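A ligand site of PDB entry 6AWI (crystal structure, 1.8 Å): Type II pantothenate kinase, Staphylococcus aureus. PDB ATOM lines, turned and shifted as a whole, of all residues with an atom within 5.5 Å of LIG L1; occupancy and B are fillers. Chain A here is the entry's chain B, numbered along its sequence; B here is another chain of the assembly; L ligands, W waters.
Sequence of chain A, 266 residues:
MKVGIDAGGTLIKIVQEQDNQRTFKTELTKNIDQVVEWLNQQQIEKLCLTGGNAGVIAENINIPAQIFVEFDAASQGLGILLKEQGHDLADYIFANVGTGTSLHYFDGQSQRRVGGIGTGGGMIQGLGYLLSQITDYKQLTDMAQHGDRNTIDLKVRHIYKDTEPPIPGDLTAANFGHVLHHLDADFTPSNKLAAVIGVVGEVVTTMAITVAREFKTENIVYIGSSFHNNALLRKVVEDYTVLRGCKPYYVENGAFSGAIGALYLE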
ATOM      1  N   VAL A 156      31.191   4.993   3.294  1.00  0.00           N
ATOM      2  CA  VAL A 156      30.175   5.770   4.006  1.00  0.00           C
ATOM      3  C   VAL A 156      30.715   7.242   4.228  1.00  0.00           C
ATOM      4  O   VAL A 156      29.993   8.206   3.987  1.00  0.00           O
ATOM      5  CB  VAL A 156      29.861   5.098   5.342  1.00  0.00           C
ATOM      6  CG1 VAL A 156      29.061   6.032   6.227  1.00  0.00           C
ATOM      7  CG2 VAL A 156      29.020   3.848   5.119  1.00  0.00           C
ATOM      8  N   ILE A 159      30.241   9.603   1.378  1.00  0.00           N
ATOM      9  CA  ILE A 159      28.859  10.142   1.157  1.00  0.00           C
ATOM     10  C   ILE A 159      28.550  11.191   2.195  1.00  0.00           C
ATOM     11  O   ILE A 159      27.935  12.201   1.880  1.00  0.00           O
ATOM     12  CB  ILE A 159      27.831   9.042   1.272  1.00  0.00           C
ATOM     13  CG1 ILE A 159      28.065   8.099   0.107  1.00  0.00           C
ATOM     14  CG2 ILE A 159      26.417   9.595   1.332  1.00  0.00           C
ATOM     15  CD1 ILE A 159      27.088   6.951   0.032  1.00  0.00           C
ATOM     16  N   TYR A 160      28.957  10.920   3.448  1.00  0.00           N
ATOM     17  CA  TYR A 160      28.765  11.837   4.562  1.00  0.00           C
ATOM     18  C   TYR A 160      29.845  12.976   4.539  1.00  0.00           C
ATOM     19  O   TYR A 160      30.759  13.019   5.294  1.00  0.00           O
ATOM     20  CB  TYR A 160      28.623  11.080   5.880  1.00  0.00           C
ATOM     21  CG  TYR A 160      27.197  10.662   6.086  1.00  0.00           C
ATOM     22  CD1 TYR A 160      26.656   9.551   5.393  1.00  0.00           C
ATOM     23  CD2 TYR A 160      26.363  11.404   6.898  1.00  0.00           C
ATOM     24  CE1 TYR A 160      25.300   9.239   5.524  1.00  0.00           C
ATOM     25  CE2 TYR A 160      25.034  11.093   7.054  1.00  0.00           C
ATOM     26  CZ  TYR A 160      24.505  10.028   6.341  1.00  0.00           C
ATOM     27  OH  TYR A 160      23.183   9.729   6.529  1.00  0.00           O
ATOM     28  N   ILE A 167      26.468   5.349  10.788  1.00  0.00           N
ATOM     29  CA  ILE A 167      27.179   4.061  10.884  1.00  0.00           C
ATOM     30  C   ILE A 167      28.661   4.310  10.568  1.00  0.00           C
ATOM     31  O   ILE A 167      29.031   5.417  10.094  1.00  0.00           O
ATOM     32  CB  ILE A 167      26.531   2.998   9.928  1.00  0.00           C
ATOM     33  CG1 ILE A 167      26.723   3.447   8.490  1.00  0.00           C
ATOM     34  CG2 ILE A 167      25.074   2.865  10.253  1.00  0.00           C
ATOM     35  CD1 ILE A 167      26.112   2.557   7.431  1.00  0.00           C
ATOM     36  N   LEU A 171      33.089   1.836   6.404  1.00  0.00           N
ATOM     37  CA  LEU A 171      32.312   0.792   5.719  1.00  0.00           C
ATOM     38  C   LEU A 171      32.160   1.131   4.253  1.00  0.00           C
ATOM     39  O   LEU A 171      32.019   2.284   3.876  1.00  0.00           O
ATOM     40  CB  LEU A 171      30.893   0.702   6.265  1.00  0.00           C
ATOM     41  CG  LEU A 171      30.630   0.069   7.605  1.00  0.00           C
ATOM     42  CD1 LEU A 171      29.168   0.223   8.016  1.00  0.00           C
ATOM     43  CD2 LEU A 171      31.008  -1.426   7.594  1.00  0.00           C
ATOM     44  N   THR A 172      32.253   0.138   3.418  1.00  0.00           N
ATOM     45  CA  THR A 172      31.881   0.283   1.988  1.00  0.00           C
ATOM     46  C   THR A 172      30.411   0.623   1.918  1.00  0.00           C
ATOM     47  O   THR A 172      29.570  -0.095   2.467  1.00  0.00           O
ATOM     48  CB  THR A 172      32.071  -1.078   1.243  1.00  0.00           C
ATOM     49  OG1 THR A 172      33.380  -1.576   1.492  1.00  0.00           O
ATOM     50  CG2 THR A 172      31.863  -0.877  -0.209  1.00  0.00           C
ATOM     51  N   ALA A 173      30.094   1.718   1.252  1.00  0.00           N
ATOM     52  CA  ALA A 173      28.735   2.176   0.998  1.00  0.00           C
ATOM     53  C   ALA A 173      28.189   1.671  -0.304  1.00  0.00           C
ATOM     54  O   ALA A 173      26.999   1.331  -0.405  1.00  0.00           O
ATOM     55  CB  ALA A 173      28.701   3.719   1.034  1.00  0.00           C
ATOM     56  N   ALA A 174      29.047   1.686  -1.328  1.00  0.00           N
ATOM     57  CA  ALA A 174      28.696   1.259  -2.675  1.00  0.00           C
ATOM     58  C   ALA A 174      29.901   0.654  -3.401  1.00  0.00           C
ATOM     59  O   ALA A 174      30.876   1.366  -3.691  1.00  0.00           O
ATOM     60  CB  ALA A 174      28.075   2.408  -3.493  1.00  0.00           C
ATOM     61  N   GLU A 202      32.385  -9.301   0.755  1.00  0.00           N
ATOM     62  CA  GLU A 202      31.472  -8.549   1.589  1.00  0.00           C
ATOM     63  C   GLU A 202      30.055  -9.093   1.536  1.00  0.00           C
ATOM     64  O   GLU A 202      29.402  -9.146   2.612  1.00  0.00           O
ATOM     65  CB  GLU A 202      31.439  -7.052   1.213  1.00  0.00           C
ATOM     66  CG  GLU A 202      32.789  -6.342   1.468  1.00  0.00           C
ATOM     67  CD  GLU A 202      32.848  -4.870   0.945  1.00  0.00           C
ATOM     68  OE1 GLU A 202      31.891  -4.375   0.257  1.00  0.00           O
ATOM     69  OE2 GLU A 202      33.899  -4.255   1.195  1.00  0.00           O
ATOM     70  N   THR A 206      28.341 -10.626   4.808  1.00  0.00           N
ATOM     71  CA  THR A 206      27.058  -9.995   5.192  1.00  0.00           C
ATOM     72  C   THR A 206      25.992 -11.051   5.383  1.00  0.00           C
ATOM     73  O   THR A 206      25.349 -11.100   6.409  1.00  0.00           O
ATOM     74  CB  THR A 206      26.605  -8.974   4.195  1.00  0.00           C
ATOM     75  OG1 THR A 206      27.574  -7.890   4.201  1.00  0.00           O
ATOM     76  CG2 THR A 206      25.240  -8.365   4.638  1.00  0.00           C
ATOM     77  N   TYR A 240      35.807  -8.354   8.249  1.00  0.00           N
ATOM     78  CA  TYR A 240      34.436  -7.879   8.408  1.00  0.00           C
ATOM     79  C   TYR A 240      33.710  -8.799   9.374  1.00  0.00           C
ATOM     80  O   TYR A 240      32.932  -8.332  10.159  1.00  0.00           O
ATOM     81  CB  TYR A 240      33.727  -7.732   7.029  1.00  0.00           C
ATOM     82  CG  TYR A 240      32.460  -6.995   7.187  1.00  0.00           C
ATOM     83  CD1 TYR A 240      32.408  -5.758   7.867  1.00  0.00           C
ATOM     84  CD2 TYR A 240      31.295  -7.526   6.752  1.00  0.00           C
ATOM     85  CE1 TYR A 240      31.200  -5.101   8.040  1.00  0.00           C
ATOM     86  CE2 TYR A 240      30.070  -6.842   6.913  1.00  0.00           C
ATOM     87  CZ  TYR A 240      30.045  -5.653   7.566  1.00  0.00           C
ATOM     88  OH  TYR A 240      28.869  -4.998   7.713  1.00  0.00           O
ATOM     89  N   GLU B  70      18.859  10.021   8.345  1.00  0.00           N
ATOM     90  CA  GLU B  70      18.107   9.560   7.216  1.00  0.00           C
ATOM     91  C   GLU B  70      17.306   8.264   7.422  1.00  0.00           C
ATOM     92  O   GLU B  70      16.300   8.044   6.690  1.00  0.00           O
ATOM     93  CB  GLU B  70      18.997   9.358   5.948  1.00  0.00           C
ATOM     94  CG  GLU B  70      20.086   8.298   6.089  1.00  0.00           C
ATOM     95  CD  GLU B  70      20.811   8.050   4.752  1.00  0.00           C
ATOM     96  OE1 GLU B  70      20.168   7.457   3.821  1.00  0.00           O
ATOM     97  OE2 GLU B  70      21.965   8.506   4.574  1.00  0.00           O
ATOM     98  N   PHE B  71      17.698   7.447   8.397  1.00  0.00           N
ATOM     99  CA  PHE B  71      16.966   6.191   8.654  1.00  0.00           C
ATOM    100  C   PHE B  71      15.581   6.512   9.276  1.00  0.00           C
ATOM    101  O   PHE B  71      14.546   5.998   8.872  1.00  0.00           O
ATOM    102  CB  PHE B  71      17.784   5.251   9.581  1.00  0.00           C
ATOM    103  CG  PHE B  71      19.184   4.952   9.081  1.00  0.00           C
ATOM    104  CD1 PHE B  71      19.444   4.823   7.715  1.00  0.00           C
ATOM    105  CD2 PHE B  71      20.256   4.769  10.031  1.00  0.00           C
ATOM    106  CE1 PHE B  71      20.721   4.581   7.261  1.00  0.00           C
ATOM    107  CE2 PHE B  71      21.522   4.473   9.574  1.00  0.00           C
ATOM    108  CZ  PHE B  71      21.745   4.404   8.164  1.00  0.00           C
ATOM    109  N   THR B  99      22.409   4.761  -3.664  1.00  0.00           N
ATOM    110  CA  THR B  99      23.754   4.609  -4.072  1.00  0.00           C
ATOM    111  C   THR B  99      24.276   3.274  -3.477  1.00  0.00           C
ATOM    112  O   THR B  99      24.928   2.471  -4.197  1.00  0.00           O
ATOM    113  CB  THR B  99      24.584   5.747  -3.517  1.00  0.00           C
ATOM    114  OG1 THR B  99      24.070   6.990  -4.055  1.00  0.00           O
ATOM    115  CG2 THR B  99      26.000   5.537  -3.978  1.00  0.00           C
ATOM    116  N   GLY B 100      23.908   3.022  -2.211  1.00  0.00           N
ATOM    117  CA  GLY B 100      24.088   1.783  -1.535  1.00  0.00           C
ATOM    118  C   GLY B 100      22.751   1.339  -0.920  1.00  0.00           C
ATOM    119  O   GLY B 100      21.786   2.086  -0.965  1.00  0.00           O
ATOM    120  N   THR B 101      22.724   0.148  -0.330  1.00  0.00           N
ATOM    121  CA  THR B 101      21.531  -0.435   0.219  1.00  0.00           C
ATOM    122  C   THR B 101      21.519  -0.600   1.763  1.00  0.00           C
ATOM    123  O   THR B 101      22.366  -1.223   2.323  1.00  0.00           O
ATOM    124  CB  THR B 101      21.243  -1.765  -0.463  1.00  0.00           C
ATOM    125  OG1 THR B 101      21.093  -1.540  -1.869  1.00  0.00           O
ATOM    126  CG2 THR B 101      19.960  -2.343   0.055  1.00  0.00           C
ATOM    127  N   SER B 102      20.473  -0.061   2.380  1.00  0.00           N
ATOM    128  CA  SER B 102      20.262  -0.101   3.801  1.00  0.00           C
ATOM    129  C   SER B 102      18.914  -0.788   4.098  1.00  0.00           C
ATOM    130  O   SER B 102      17.880  -0.538   3.374  1.00  0.00           O
ATOM    131  CB  SER B 102      20.357   1.348   4.325  1.00  0.00           C
ATOM    132  OG  SER B 102      20.177   1.407   5.709  1.00  0.00           O
ATOM    133  N   ARG B 113      17.692  -0.328  11.966  1.00  0.00           N
ATOM    134  CA  ARG B 113      18.516  -0.813  10.830  1.00  0.00           C
ATOM    135  C   ARG B 113      19.030  -2.222  11.202  1.00  0.00           C
ATOM    136  O   ARG B 113      19.564  -2.440  12.297  1.00  0.00           O
ATOM    137  CB  ARG B 113      19.627   0.221  10.560  1.00  0.00           C
ATOM    138  CG  ARG B 113      20.526  -0.097   9.389  1.00  0.00           C
ATOM    139  CD  ARG B 113      21.454   1.046   9.017  1.00  0.00           C
ATOM    140  NE  ARG B 113      22.144   0.836   7.720  1.00  0.00           N
ATOM    141  CZ  ARG B 113      23.189   0.072   7.475  1.00  0.00           C
ATOM    142  NH1 ARG B 113      23.721  -0.711   8.384  1.00  0.00           N
ATOM    143  NH2 ARG B 113      23.652   0.043   6.249  1.00  0.00           N
ATOM    144  N   GLY B 115      20.550  -4.359   8.551  1.00  0.00           N
ATOM    145  CA  GLY B 115      21.724  -4.675   7.728  1.00  0.00           C
ATOM    146  C   GLY B 115      21.918  -3.661   6.619  1.00  0.00           C
ATOM    147  O   GLY B 115      21.190  -2.644   6.524  1.00  0.00           O
ATOM    148  N   GLY B 116      22.917  -3.922   5.793  1.00  0.00           N
ATOM    149  CA  GLY B 116      23.144  -3.140   4.591  1.00  0.00           C
ATOM    150  C   GLY B 116      24.163  -3.846   3.783  1.00  0.00           C
ATOM    151  O   GLY B 116      24.886  -4.708   4.302  1.00  0.00           O
ATOM    152  N   ILE B 117      24.305  -3.397   2.570  1.00  0.00           N
ATOM    153  CA  ILE B 117      25.228  -3.966   1.660  1.00  0.00           C
ATOM    154  C   ILE B 117      25.550  -2.925   0.592  1.00  0.00           C
ATOM    155  O   ILE B 117      24.741  -2.042   0.270  1.00  0.00           O
ATOM    156  CB  ILE B 117      24.624  -5.249   1.089  1.00  0.00           C
ATOM    157  CG1 ILE B 117      25.651  -6.008   0.223  1.00  0.00           C
ATOM    158  CG2 ILE B 117      23.336  -5.024   0.347  1.00  0.00           C
ATOM    159  CD1 ILE B 117      26.580  -6.792   1.066  1.00  0.00           C
ATOM    160  N   GLY B 118      26.744  -3.034   0.023  1.00  0.00           N
ATOM    161  CA  GLY B 118      27.148  -2.101  -1.026  1.00  0.00           C
ATOM    162  C   GLY B 118      26.647  -2.369  -2.419  1.00  0.00           C
ATOM    163  O   GLY B 118      27.032  -1.672  -3.353  1.00  0.00           O
HETATM  164  C1  LIG L   1      23.801   6.121   2.680  1.00  0.00           C
HETATM  165  C2  LIG L   1      24.084   4.755   3.345  1.00  0.00           C
HETATM  166  C3  LIG L   1      23.224   4.631   4.667  1.00  0.00           C
HETATM  167  C4  LIG L   1      25.588   4.682   3.732  1.00  0.00           C
HETATM  168  C5  LIG L   1      23.775   3.566   2.345  1.00  0.00           C
HETATM  169  O1  LIG L   1      24.437   3.787   1.113  1.00  0.00           O
HETATM  170  C6  LIG L   1      24.154   2.219   2.923  1.00  0.00           C
HETATM  171  O2  LIG L   1      23.594   1.833   3.957  1.00  0.00           O
HETATM  172  N1  LIG L   1      25.225   1.602   2.360  1.00  0.00           N
HETATM  173  C7  LIG L   1      25.691   0.285   2.779  1.00  0.00           C
HETATM  174  C8  LIG L   1      26.570   0.359   4.049  1.00  0.00           C
HETATM  175  C9  LIG L   1      26.751  -1.019   4.636  1.00  0.00           C
HETATM  176  O3  LIG L   1      25.999  -1.463   5.524  1.00  0.00           O
HETATM  177  N2  LIG L   1      27.796  -1.715   4.165  1.00  0.00           N
HETATM  178  C10 LIG L   1      28.016  -3.109   4.565  1.00  0.00           C
HETATM  179  C11 LIG L   1      29.095  -3.748   3.718  1.00  0.00           C
HETATM  180  C12 LIG L   1      30.353  -3.481   4.529  1.00  0.00           C
HETATM  181  C13 LIG L   1      31.300  -4.533   4.273  1.00  0.00           C
HETATM  182  C14 LIG L   1      32.697  -3.972   4.558  1.00  0.00           C
HETATM  183  P1  LG2 L   2      21.126   8.381  -2.750  1.00  0.00           P
HETATM  184  O1  LG2 L   2      22.202   7.514  -2.165  1.00  0.00           O
HETATM  185  O2  LG2 L   2      21.612   9.439  -3.682  1.00  0.00           O
HETATM  186  O3  LG2 L   2      20.171   8.861  -1.693  1.00  0.00           O
HETATM  187  P2  LG2 L   2      18.916   7.294  -4.384  1.00  0.00           P
HETATM  188  O4  LG2 L   2      17.864   6.486  -3.700  1.00  0.00           O
HETATM  189  O5  LG2 L   2      18.595   8.663  -4.858  1.00  0.00           O
HETATM  190  O6  LG2 L   2      20.317   7.265  -3.552  1.00  0.00           O
HETATM  191  O7  LG2 L   2      19.406   6.302  -5.544  1.00  0.00           O
HETATM  192  C1  LG2 L   2      20.563   6.551  -6.329  1.00  0.00           C
HETATM  193  C2  LG2 L   2      20.559   5.710  -7.574  1.00  0.00           C
HETATM  194  O8  LG2 L   2      19.411   5.865  -8.356  1.00  0.00           O
HETATM  195  C3  LG2 L   2      21.658   5.899  -8.606  1.00  0.00           C
HETATM  196  O9  LG2 L   2      22.826   5.224  -8.006  1.00  0.00           O
HETATM  197  C4  LG2 L   2      21.096   5.253  -9.841  1.00  0.00           C
HETATM  198  O10 LG2 L   2      21.244   3.832  -9.785  1.00  0.00           O
HETATM  199  C5  LG2 L   2      19.599   5.537  -9.714  1.00  0.00           C
HETATM  200  N1  LG2 L   2      19.163   6.736 -10.533  1.00  0.00           N
HETATM  201  C6  LG2 L   2      17.870   6.999 -10.764  1.00  0.00           C
HETATM  202  N2  LG2 L   2      17.713   8.106 -11.511  1.00  0.00           N
HETATM  203  C7  LG2 L   2      18.921   8.606 -11.712  1.00  0.00           C
HETATM  204  C8  LG2 L   2      19.505   9.731 -12.434  1.00  0.00           C
HETATM  205  N3  LG2 L   2      18.701  10.640 -13.076  1.00  0.00           N
HETATM  206  N4  LG2 L   2      20.815   9.895 -12.437  1.00  0.00           N
HETATM  207  C9  LG2 L   2      21.662   9.091 -11.794  1.00  0.00           C
HETATM  208  N5  LG2 L   2      21.161   8.040 -11.151  1.00  0.00           N
HETATM  209  C10 LG2 L   2      19.862   7.726 -11.064  1.00  0.00           C
HETATM  210  O   HOH W   1      26.867  -5.884   5.999  1.00  0.00           O
HETATM  211  O   HOH W   2      23.185   7.992   0.111  1.00  0.00           O
HETATM  212  O   HOH W   3      25.652  -2.787   7.810  1.00  0.00           O
HETATM  213  O   HOH W   4      22.613   4.929  -0.321  1.00  0.00           O
HETATM  214  O   HOH W   5      34.746  -1.286   4.751  1.00  0.00           O
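The side-chain hydroxyl of Thr 99 of chain B sits at hydrogen-bond distance from an oxygen (O1) of LG2 L2. N of Gly 100 of chain B lies close to O1 of LIG L1 (3.5 Å). The backbone NH of Thr 99 of chain B lies within hydrogen-bond range of an oxygen (O1) of LG2 L2. O of Thr 172 sits at hydrogen-bond distance from N2 of LIG L1. An oxygen (O3) of LIG L1 sits at hydrogen-bond distance from the guanidinium group (NH2) of Arg 113 of chain B. A nitrogen (N1) of LIG L1 sits at hydrogen-bond distance from the backbone carbonyl oxygen of Ala 173, 3.3 Å away.
Merely in contact with LIG L1: Ser 102 of chain B (3.3 Å), Gly 116 of chain B (3.4 Å), Ile 117 of chain B (3.6 Å), Glu 70 of chain B (3.6 Å), Glu 202 (3.6 Å), Phe 71 of chain B (3.6 Å), Thr 101 of chain B (3.7 Å), Tyr 240 (3.7 Å), Leu 171 (3.7 Å) and Val 156 (3.8 Å). Of the 22 residues printed, 14 come within 4 Å of LIG L1.
OE2 of Glu 202 sits at hydrogen-bond distance from OG1 of Thr 172 (2.7 Å). The backbone carbonyl oxygen of Glu 202 is in hydrogen-bond range of the side-chain hydroxyl of Thr 206 (2.7 Å). OE2 of Glu 70 of chain B sits at hydrogen-bond distance from OH of Tyr 160, 2.6 Å away. The backbone NH (N) of Val 156 sits at hydrogen-bond distance from the backbone carbonyl oxygen (O) of Leu 171 (2.9 Å). O of Thr 101 of chain B lies within hydrogen-bond range of N of Ile 117 of chain B (2.9 Å). The side-chain hydroxyl (OG) of Ser 102 of chain B sits at hydrogen-bond distance from the guanidinium group (NE) of Arg 113 of chain B (2.9 Å).
Water W4 lies within hydrogen-bond range of O1 of LIG L1 (2.6 Å), N of Gly 100 of chain B (3.0 Å), O1 of LG2 L2 (3.2 Å) and N of Thr 99 of chain B (3.4 Å). Water W3 bridges O3 of LIG L1 and NH1 of Arg 113 of chain B. Water W1 lies within hydrogen-bond range of the side-chain hydroxyl (OH) of Tyr 240, the side-chain hydroxyl (OG1) of Thr 206 and the backbone carbonyl oxygen (O) of Gly 116 of chain B.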
